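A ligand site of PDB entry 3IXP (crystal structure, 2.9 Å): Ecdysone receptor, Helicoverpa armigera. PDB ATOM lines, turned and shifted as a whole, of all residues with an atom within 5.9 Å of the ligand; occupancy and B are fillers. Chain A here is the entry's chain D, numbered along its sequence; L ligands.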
ATOM      1  N   PHE A  69       7.698  11.011  25.414  1.00  0.00           N
ATOM      2  CA  PHE A  69       8.652  10.008  24.931  1.00  0.00           C
ATOM      3  C   PHE A  69       8.973  10.237  23.458  1.00  0.00           C
ATOM      4  O   PHE A  69      10.088   9.936  23.005  1.00  0.00           O
ATOM      5  CB  PHE A  69       8.056   8.608  25.110  1.00  0.00           C
ATOM      6  CG  PHE A  69       8.992   7.493  24.745  1.00  0.00           C
ATOM      7  CD1 PHE A  69      10.073   7.174  25.562  1.00  0.00           C
ATOM      8  CD2 PHE A  69       8.776   6.740  23.591  1.00  0.00           C
ATOM      9  CE1 PHE A  69      10.931   6.123  25.232  1.00  0.00           C
ATOM     10  CE2 PHE A  69       9.634   5.689  23.261  1.00  0.00           C
ATOM     11  CZ  PHE A  69      10.710   5.376  24.085  1.00  0.00           C
ATOM     12  N   ILE A  72      12.051  13.054  23.276  1.00  0.00           N
ATOM     13  CA  ILE A  72      13.286  12.380  23.664  1.00  0.00           C
ATOM     14  C   ILE A  72      13.850  11.527  22.536  1.00  0.00           C
ATOM     15  O   ILE A  72      14.841  11.896  21.907  1.00  0.00           O
ATOM     16  CB  ILE A  72      13.044  11.472  24.899  1.00  0.00           C
ATOM     17  CG1 ILE A  72      12.479  12.296  26.056  1.00  0.00           C
ATOM     18  CG2 ILE A  72      14.348  10.818  25.321  1.00  0.00           C
ATOM     19  CD1 ILE A  72      12.157  11.482  27.280  1.00  0.00           C
ATOM     20  N   THR A  73      13.200  10.405  22.279  1.00  0.00           N
ATOM     21  CA  THR A  73      13.622   9.475  21.230  1.00  0.00           C
ATOM     22  C   THR A  73      14.134  10.144  19.946  1.00  0.00           C
ATOM     23  O   THR A  73      15.021   9.599  19.272  1.00  0.00           O
ATOM     24  CB  THR A  73      12.469   8.511  20.863  1.00  0.00           C
ATOM     25  OG1 THR A  73      11.267   9.252  20.658  1.00  0.00           O
ATOM     26  CG2 THR A  73      12.258   7.488  21.961  1.00  0.00           C
ATOM     27  N   THR A  76      17.464  12.406  20.924  1.00  0.00           N
ATOM     28  CA  THR A  76      18.556  11.480  21.167  1.00  0.00           C
ATOM     29  C   THR A  76      19.177  11.092  19.837  1.00  0.00           C
ATOM     30  O   THR A  76      20.403  11.137  19.671  1.00  0.00           O
ATOM     31  CB  THR A  76      18.075  10.215  21.881  1.00  0.00           C
ATOM     32  OG1 THR A  76      17.773  10.536  23.249  1.00  0.00           O
ATOM     33  CG2 THR A  76      19.131   9.130  21.836  1.00  0.00           C
ATOM     34  N   SER A 109      27.746   4.736  22.203  1.00  0.00           N
ATOM     35  CA  SER A 109      26.628   5.663  22.020  1.00  0.00           C
ATOM     36  C   SER A 109      25.897   6.112  23.283  1.00  0.00           C
ATOM     37  O   SER A 109      25.741   7.309  23.506  1.00  0.00           O
ATOM     38  CB  SER A 109      25.622   5.072  21.016  1.00  0.00           C
ATOM     39  OG  SER A 109      25.211   3.781  21.406  1.00  0.00           O
ATOM     40  N   SER A 110      25.457   5.183  24.128  1.00  0.00           N
ATOM     41  CA  SER A 110      24.747   5.578  25.331  1.00  0.00           C
ATOM     42  C   SER A 110      25.689   6.202  26.335  1.00  0.00           C
ATOM     43  O   SER A 110      25.364   7.220  26.964  1.00  0.00           O
ATOM     44  CB  SER A 110      24.046   4.369  25.982  1.00  0.00           C
ATOM     45  OG  SER A 110      24.960   3.570  26.719  1.00  0.00           O
ATOM     46  N   MET A 113      26.475   9.576  25.437  1.00  0.00           N
ATOM     47  CA  MET A 113      25.230  10.341  25.531  1.00  0.00           C
ATOM     48  C   MET A 113      25.131  10.898  26.947  1.00  0.00           C
ATOM     49  O   MET A 113      24.782  12.061  27.167  1.00  0.00           O
ATOM     50  CB  MET A 113      24.039   9.411  25.277  1.00  0.00           C
ATOM     51  CG  MET A 113      23.495   9.388  23.860  1.00  0.00           C
ATOM     52  SD  MET A 113      22.221  10.633  23.673  1.00  0.00           S
ATOM     53  CE  MET A 113      23.203  12.033  23.111  1.00  0.00           C
ATOM     54  N   MET A 114      25.445  10.041  27.911  1.00  0.00           N
ATOM     55  CA  MET A 114      25.435  10.383  29.337  1.00  0.00           C
ATOM     56  C   MET A 114      26.385  11.565  29.571  1.00  0.00           C
ATOM     57  O   MET A 114      26.078  12.484  30.314  1.00  0.00           O
ATOM     58  CB  MET A 114      25.892   9.166  30.145  1.00  0.00           C
ATOM     59  CG  MET A 114      25.000   8.784  31.316  1.00  0.00           C
ATOM     60  SD  MET A 114      23.334   8.256  30.839  1.00  0.00           S
ATOM     61  CE  MET A 114      23.652   7.626  29.197  1.00  0.00           C
ATOM     62  N   VAL A 117      24.819  14.989  28.118  1.00  0.00           N
ATOM     63  CA  VAL A 117      23.837  15.550  29.042  1.00  0.00           C
ATOM     64  C   VAL A 117      24.521  16.074  30.286  1.00  0.00           C
ATOM     65  O   VAL A 117      24.363  17.233  30.659  1.00  0.00           O
ATOM     66  CB  VAL A 117      22.791  14.521  29.454  1.00  0.00           C
ATOM     67  CG1 VAL A 117      22.031  15.009  30.655  1.00  0.00           C
ATOM     68  CG2 VAL A 117      21.824  14.312  28.320  1.00  0.00           C
ATOM     69  N   TYR A 136      14.998  16.668  28.110  1.00  0.00           N
ATOM     70  CA  TYR A 136      15.837  16.096  29.143  1.00  0.00           C
ATOM     71  C   TYR A 136      15.622  16.806  30.476  1.00  0.00           C
ATOM     72  O   TYR A 136      16.579  17.142  31.182  1.00  0.00           O
ATOM     73  CB  TYR A 136      17.309  16.166  28.720  1.00  0.00           C
ATOM     74  CG  TYR A 136      17.640  15.432  27.436  1.00  0.00           C
ATOM     75  CD1 TYR A 136      18.778  15.750  26.698  1.00  0.00           C
ATOM     76  CD2 TYR A 136      16.802  14.424  26.951  1.00  0.00           C
ATOM     77  CE1 TYR A 136      19.077  15.073  25.509  1.00  0.00           C
ATOM     78  CE2 TYR A 136      17.095  13.747  25.774  1.00  0.00           C
ATOM     79  CZ  TYR A 136      18.231  14.078  25.053  1.00  0.00           C
ATOM     80  OH  TYR A 136      18.523  13.414  23.894  1.00  0.00           O
ATOM     81  N   TYR A 141      10.491  13.698  31.440  1.00  0.00           N
ATOM     82  CA  TYR A 141      10.837  12.331  31.827  1.00  0.00           C
ATOM     83  C   TYR A 141       9.760  11.734  32.717  1.00  0.00           C
ATOM     84  O   TYR A 141       9.667  10.517  32.873  1.00  0.00           O
ATOM     85  CB  TYR A 141      12.203  12.279  32.530  1.00  0.00           C
ATOM     86  CG  TYR A 141      13.320  11.864  31.595  1.00  0.00           C
ATOM     87  CD1 TYR A 141      13.797  12.737  30.626  1.00  0.00           C
ATOM     88  CD2 TYR A 141      13.853  10.585  31.650  1.00  0.00           C
ATOM     89  CE1 TYR A 141      14.789  12.343  29.719  1.00  0.00           C
ATOM     90  CE2 TYR A 141      14.832  10.174  30.750  1.00  0.00           C
ATOM     91  CZ  TYR A 141      15.299  11.060  29.793  1.00  0.00           C
ATOM     92  OH  TYR A 141      16.274  10.655  28.916  1.00  0.00           O
ATOM     93  N   MET A 146       9.313   7.367  32.486  1.00  0.00           N
ATOM     94  CA  MET A 146      10.652   7.112  33.016  1.00  0.00           C
ATOM     95  C   MET A 146      11.189   8.277  33.838  1.00  0.00           C
ATOM     96  O   MET A 146      12.119   8.970  33.418  1.00  0.00           O
ATOM     97  CB  MET A 146      11.593   6.798  31.858  1.00  0.00           C
ATOM     98  CG  MET A 146      11.557   7.864  30.785  1.00  0.00           C
ATOM     99  SD  MET A 146      12.383   7.305  29.300  1.00  0.00           S
ATOM    100  CE  MET A 146      11.091   6.300  28.608  1.00  0.00           C
ATOM    101  N   VAL A 149      14.441   7.166  36.632  1.00  0.00           N
ATOM    102  CA  VAL A 149      15.787   7.309  36.103  1.00  0.00           C
ATOM    103  C   VAL A 149      16.450   8.678  36.330  1.00  0.00           C
ATOM    104  O   VAL A 149      17.686   8.772  36.348  1.00  0.00           O
ATOM    105  CB  VAL A 149      15.777   6.971  34.591  1.00  0.00           C
ATOM    106  CG1 VAL A 149      16.560   7.982  33.801  1.00  0.00           C
ATOM    107  CG2 VAL A 149      16.347   5.581  34.382  1.00  0.00           C
ATOM    108  N   ASP A 152      19.248   9.007  39.323  1.00  0.00           N
ATOM    109  CA  ASP A 152      20.522   8.373  38.990  1.00  0.00           C
ATOM    110  C   ASP A 152      21.293   9.234  37.986  1.00  0.00           C
ATOM    111  O   ASP A 152      22.516   9.374  38.092  1.00  0.00           O
ATOM    112  CB  ASP A 152      20.300   6.964  38.415  1.00  0.00           C
ATOM    113  CG  ASP A 152      19.950   5.939  39.489  1.00  0.00           C
ATOM    114  OD1 ASP A 152      20.270   6.186  40.669  1.00  0.00           O
ATOM    115  OD2 ASP A 152      19.370   4.881  39.157  1.00  0.00           O
ATOM    116  N   LEU A 153      20.602   9.824  37.016  1.00  0.00           N
ATOM    117  CA  LEU A 153      21.243  10.676  36.034  1.00  0.00           C
ATOM    118  C   LEU A 153      21.845  11.935  36.666  1.00  0.00           C
ATOM    119  O   LEU A 153      23.012  12.264  36.441  1.00  0.00           O
ATOM    120  CB  LEU A 153      20.263  11.103  34.943  1.00  0.00           C
ATOM    121  CG  LEU A 153      20.901  12.041  33.903  1.00  0.00           C
ATOM    122  CD1 LEU A 153      21.936  11.273  33.085  1.00  0.00           C
ATOM    123  CD2 LEU A 153      19.835  12.630  32.986  1.00  0.00           C
ATOM    124  N   LEU A 233      25.770   3.288  33.830  1.00  0.00           N
ATOM    125  CA  LEU A 233      24.712   4.082  33.197  1.00  0.00           C
ATOM    126  C   LEU A 233      24.318   3.437  31.878  1.00  0.00           C
ATOM    127  O   LEU A 233      23.131   3.386  31.531  1.00  0.00           O
ATOM    128  CB  LEU A 233      25.203   5.507  32.911  1.00  0.00           C
ATOM    129  CG  LEU A 233      25.198   6.523  34.048  1.00  0.00           C
ATOM    130  CD1 LEU A 233      24.981   5.840  35.414  1.00  0.00           C
ATOM    131  CD2 LEU A 233      26.502   7.290  34.004  1.00  0.00           C
ATOM    132  N   GLN A 236      22.071   0.471  32.561  1.00  0.00           N
ATOM    133  CA  GLN A 236      20.756   1.011  32.909  1.00  0.00           C
ATOM    134  C   GLN A 236      19.997   1.436  31.667  1.00  0.00           C
ATOM    135  O   GLN A 236      18.772   1.302  31.601  1.00  0.00           O
ATOM    136  CB  GLN A 236      20.914   2.188  33.848  1.00  0.00           C
ATOM    137  CG  GLN A 236      21.349   1.776  35.232  1.00  0.00           C
ATOM    138  CD  GLN A 236      21.674   2.946  36.111  1.00  0.00           C
ATOM    139  OE1 GLN A 236      22.672   3.634  35.912  1.00  0.00           O
ATOM    140  NE2 GLN A 236      20.826   3.178  37.100  1.00  0.00           N
ATOM    141  N   ASN A 237      20.723   1.944  30.678  1.00  0.00           N
ATOM    142  CA  ASN A 237      20.109   2.351  29.435  1.00  0.00           C
ATOM    143  C   ASN A 237      19.574   1.097  28.769  1.00  0.00           C
ATOM    144  O   ASN A 237      18.428   1.047  28.356  1.00  0.00           O
ATOM    145  CB  ASN A 237      21.115   3.029  28.523  1.00  0.00           C
ATOM    146  CG  ASN A 237      20.497   3.443  27.205  1.00  0.00           C
ATOM    147  OD1 ASN A 237      19.524   4.192  27.185  1.00  0.00           O
ATOM    148  ND2 ASN A 237      21.075   2.972  26.105  1.00  0.00           N
ATOM    149  N   SER A 238      20.433   0.078  28.683  1.00  0.00           N
ATOM    150  CA  SER A 238      20.072  -1.210  28.090  1.00  0.00           C
ATOM    151  C   SER A 238      18.851  -1.786  28.765  1.00  0.00           C
ATOM    152  O   SER A 238      17.902  -2.215  28.109  1.00  0.00           O
ATOM    153  CB  SER A 238      21.213  -2.205  28.212  1.00  0.00           C
ATOM    154  OG  SER A 238      22.250  -1.916  27.297  1.00  0.00           O
ATOM    155  N   MET A 240      16.483  -0.335  30.292  1.00  0.00           N
ATOM    156  CA  MET A 240      15.263   0.377  29.909  1.00  0.00           C
ATOM    157  C   MET A 240      14.754  -0.123  28.564  1.00  0.00           C
ATOM    158  O   MET A 240      13.549  -0.302  28.381  1.00  0.00           O
ATOM    159  CB  MET A 240      15.504   1.877  29.822  1.00  0.00           C
ATOM    160  CG  MET A 240      14.293   2.621  29.317  1.00  0.00           C
ATOM    161  SD  MET A 240      14.157   4.267  29.990  1.00  0.00           S
ATOM    162  CE  MET A 240      13.567   3.888  31.635  1.00  0.00           C
ATOM    163  N   CYS A 241      15.672  -0.321  27.628  1.00  0.00           N
ATOM    164  CA  CYS A 241      15.292  -0.806  26.320  1.00  0.00           C
ATOM    165  C   CYS A 241      14.598  -2.143  26.506  1.00  0.00           C
ATOM    166  O   CYS A 241      13.515  -2.368  25.978  1.00  0.00           O
ATOM    167  CB  CYS A 241      16.525  -0.979  25.440  1.00  0.00           C
ATOM    168  SG  CYS A 241      17.221   0.593  24.953  1.00  0.00           S
ATOM    169  N   LEU A 244      11.052  -1.531  27.616  1.00  0.00           N
ATOM    170  CA  LEU A 244      10.127  -1.110  26.572  1.00  0.00           C
ATOM    171  C   LEU A 244       9.696  -2.343  25.788  1.00  0.00           C
ATOM    172  O   LEU A 244       8.553  -2.465  25.368  1.00  0.00           O
ATOM    173  CB  LEU A 244      10.803  -0.094  25.662  1.00  0.00           C
ATOM    174  CG  LEU A 244      11.458   1.078  26.406  1.00  0.00           C
ATOM    175  CD1 LEU A 244      12.099   2.017  25.401  1.00  0.00           C
ATOM    176  CD2 LEU A 244      10.414   1.795  27.254  1.00  0.00           C
ATOM    177  N   LEU A 251      10.348   2.325  19.916  1.00  0.00           N
ATOM    178  CA  LEU A 251      11.717   2.817  19.860  1.00  0.00           C
ATOM    179  C   LEU A 251      12.087   2.933  18.378  1.00  0.00           C
ATOM    180  O   LEU A 251      12.302   1.911  17.716  1.00  0.00           O
ATOM    181  CB  LEU A 251      12.667   1.852  20.583  1.00  0.00           C
ATOM    182  CG  LEU A 251      13.837   2.490  21.343  1.00  0.00           C
ATOM    183  CD1 LEU A 251      13.295   3.195  22.574  1.00  0.00           C
ATOM    184  CD2 LEU A 251      14.863   1.450  21.747  1.00  0.00           C
ATOM    185  N   LEU A 255      17.391   3.680  16.974  1.00  0.00           N
ATOM    186  CA  LEU A 255      17.847   3.202  18.264  1.00  0.00           C
ATOM    187  C   LEU A 255      17.632   1.705  18.366  1.00  0.00           C
ATOM    188  O   LEU A 255      18.483   0.971  18.877  1.00  0.00           O
ATOM    189  CB  LEU A 255      17.061   3.909  19.370  1.00  0.00           C
ATOM    190  CG  LEU A 255      16.933   5.419  19.167  1.00  0.00           C
ATOM    191  CD1 LEU A 255      16.101   5.996  20.288  1.00  0.00           C
ATOM    192  CD2 LEU A 255      18.297   6.060  19.118  1.00  0.00           C
ATOM    193  N   TRP A 259      20.987   0.119  19.616  1.00  0.00           N
ATOM    194  CA  TRP A 259      20.974  -0.435  20.959  1.00  0.00           C
ATOM    195  C   TRP A 259      20.381  -1.839  21.016  1.00  0.00           C
ATOM    196  O   TRP A 259      19.900  -2.269  22.067  1.00  0.00           O
ATOM    197  CB  TRP A 259      20.215   0.480  21.924  1.00  0.00           C
ATOM    198  CG  TRP A 259      20.835   1.850  22.085  1.00  0.00           C
ATOM    199  CD1 TRP A 259      22.155   2.183  21.958  1.00  0.00           C
ATOM    200  CD2 TRP A 259      20.158   3.046  22.488  1.00  0.00           C
ATOM    201  NE1 TRP A 259      22.341   3.510  22.264  1.00  0.00           N
ATOM    202  CE2 TRP A 259      21.129   4.069  22.592  1.00  0.00           C
ATOM    203  CE3 TRP A 259      18.832   3.363  22.779  1.00  0.00           C
ATOM    204  CZ2 TRP A 259      20.818   5.366  22.966  1.00  0.00           C
ATOM    205  CZ3 TRP A 259      18.516   4.666  23.159  1.00  0.00           C
ATOM    206  CH2 TRP A 259      19.507   5.642  23.244  1.00  0.00           C
HETATM  207  C1  LIG L   1      18.780  10.620  26.986  1.00  0.00           C
HETATM  208  C2  LIG L   1      19.753  11.507  27.536  1.00  0.00           C
HETATM  209  C3  LIG L   1      21.070  11.014  27.853  1.00  0.00           C
HETATM  210  C4  LIG L   1      21.412   9.649  27.605  1.00  0.00           C
HETATM  211  C5  LIG L   1      20.450   8.771  27.054  1.00  0.00           C
HETATM  212  C6  LIG L   1      19.107   9.238  26.727  1.00  0.00           C
HETATM  213  C7  LIG L   1      18.043   8.350  26.172  1.00  0.00           C
HETATM  214 CL1  LIG L   1      20.979   7.138  26.801  1.00  0.00          CL
HETATM  215  N1  LIG L   1      17.497   8.481  24.971  1.00  0.00           N
HETATM  216  C8  LIG L   1      16.513   7.413  24.821  1.00  0.00           C
HETATM  217  C9  LIG L   1      16.502   6.662  25.962  1.00  0.00           C
HETATM  218  N2  LIG L   1      17.519   7.307  26.855  1.00  0.00           N
HETATM  219  C10 LIG L   1      15.703   7.291  23.559  1.00  0.00           C
HETATM  220  C11 LIG L   1      15.632   5.443  26.232  1.00  0.00           C
HETATM  221  N3  LIG L   1      17.950   7.070  28.043  1.00  0.00           N
HETATM  222  C12 LIG L   1      17.302   7.420  29.195  1.00  0.00           C
HETATM  223  C13 LIG L   1      14.361   5.813  26.964  1.00  0.00           C
HETATM  224  C14 LIG L   1      16.407   4.383  26.997  1.00  0.00           C
HETATM  225  O1  LIG L   1      16.210   7.948  29.178  1.00  0.00           O
HETATM  226  C15 LIG L   1      18.100   7.254  30.400  1.00  0.00           C
HETATM  227  C16 LIG L   1      18.717   8.505  30.793  1.00  0.00           C
HETATM  228  C17 LIG L   1      19.546   8.604  31.932  1.00  0.00           C
HETATM  229  C18 LIG L   1      19.791   7.472  32.716  1.00  0.00           C
HETATM  230  C19 LIG L   1      19.193   6.202  32.374  1.00  0.00           C
HETATM  231  C20 LIG L   1      18.331   6.062  31.203  1.00  0.00           C
HETATM  232  C21 LIG L   1      17.729   4.712  30.889  1.00  0.00           C
HETATM  233  O2  LIG L   1      20.611   7.634  33.833  1.00  0.00           O
HETATM  234  C22 LIG L   1      21.018   6.445  34.541  1.00  0.00           C
HETATM  235  C23 LIG L   1      19.900   5.352  34.541  1.00  0.00           C
HETATM  236  O3  LIG L   1      19.464   5.074  33.191  1.00  0.00           O
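The side-chain hydroxyl (OH) of Tyr 141 lies within hydrogen-bond range of an oxygen (O1) of the ligand, 2.7 Å away.
A nitrogen (N1) of the ligand sits at hydrogen-bond distance from the side-chain hydroxyl (OG1) of Thr 76, at 2.7 Å.
OD1 of Asn 237 lies close to N3 of the ligand (3.4 Å).
Residues that only touch the ligand: Gln 236 (3.3 Å), Val 149 (3.4 Å), Met 240 (3.4 Å), Met 146 (3.4 Å), Met 114 (3.4 Å), Val 117 (3.4 Å), Met 113 (3.5 Å), Leu 255 (3.5 Å), Leu 153 (3.7 Å), Tyr 136 (3.8 Å), Trp 259 (3.8 Å), Thr 73 (3.8 Å), Phe 69 (3.9 Å), Ile 72 (3.9 Å) and Asp 152 (3.97 Å).
Hydrophobic or aromatic side chains within 4 Å of the ligand: Phe 69, Ile 72, Met 113, Met 114, Val 117, Tyr 136, Tyr 141, Met 146, Val 149, Leu 153, Met 240, Leu 255 and Trp 259.
The nearest printed residue that does not touch the ligand is Leu 233 (4.1 Å).
OG1 of Thr 76 sits at hydrogen-bond distance from O of Ile 72 (3.5 Å).
OD2 of Asp 152 is in hydrogen-bond range of NE2 of Gln 236 (3.0 Å).
The backbone carbonyl oxygen of Tyr 141 sits close to the backbone NH of Met 146 (3.2 Å).
OH of Tyr 136 lies within hydrogen-bond range of OG1 of Thr 76, at 3.0 Å.
O of Asn 237 lies within hydrogen-bond range of SG of Cys 241 (3.6 Å).
The side-chain hydroxyl (OG) of Ser 109 sits at hydrogen-bond distance from the indole nitrogen (NE1) of Trp 259 (3.0 Å).
The backbone carbonyl oxygen (O) of Phe 69 is in hydrogen-bond range of the side-chain hydroxyl (OG1) of Thr 73 (2.7 Å).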
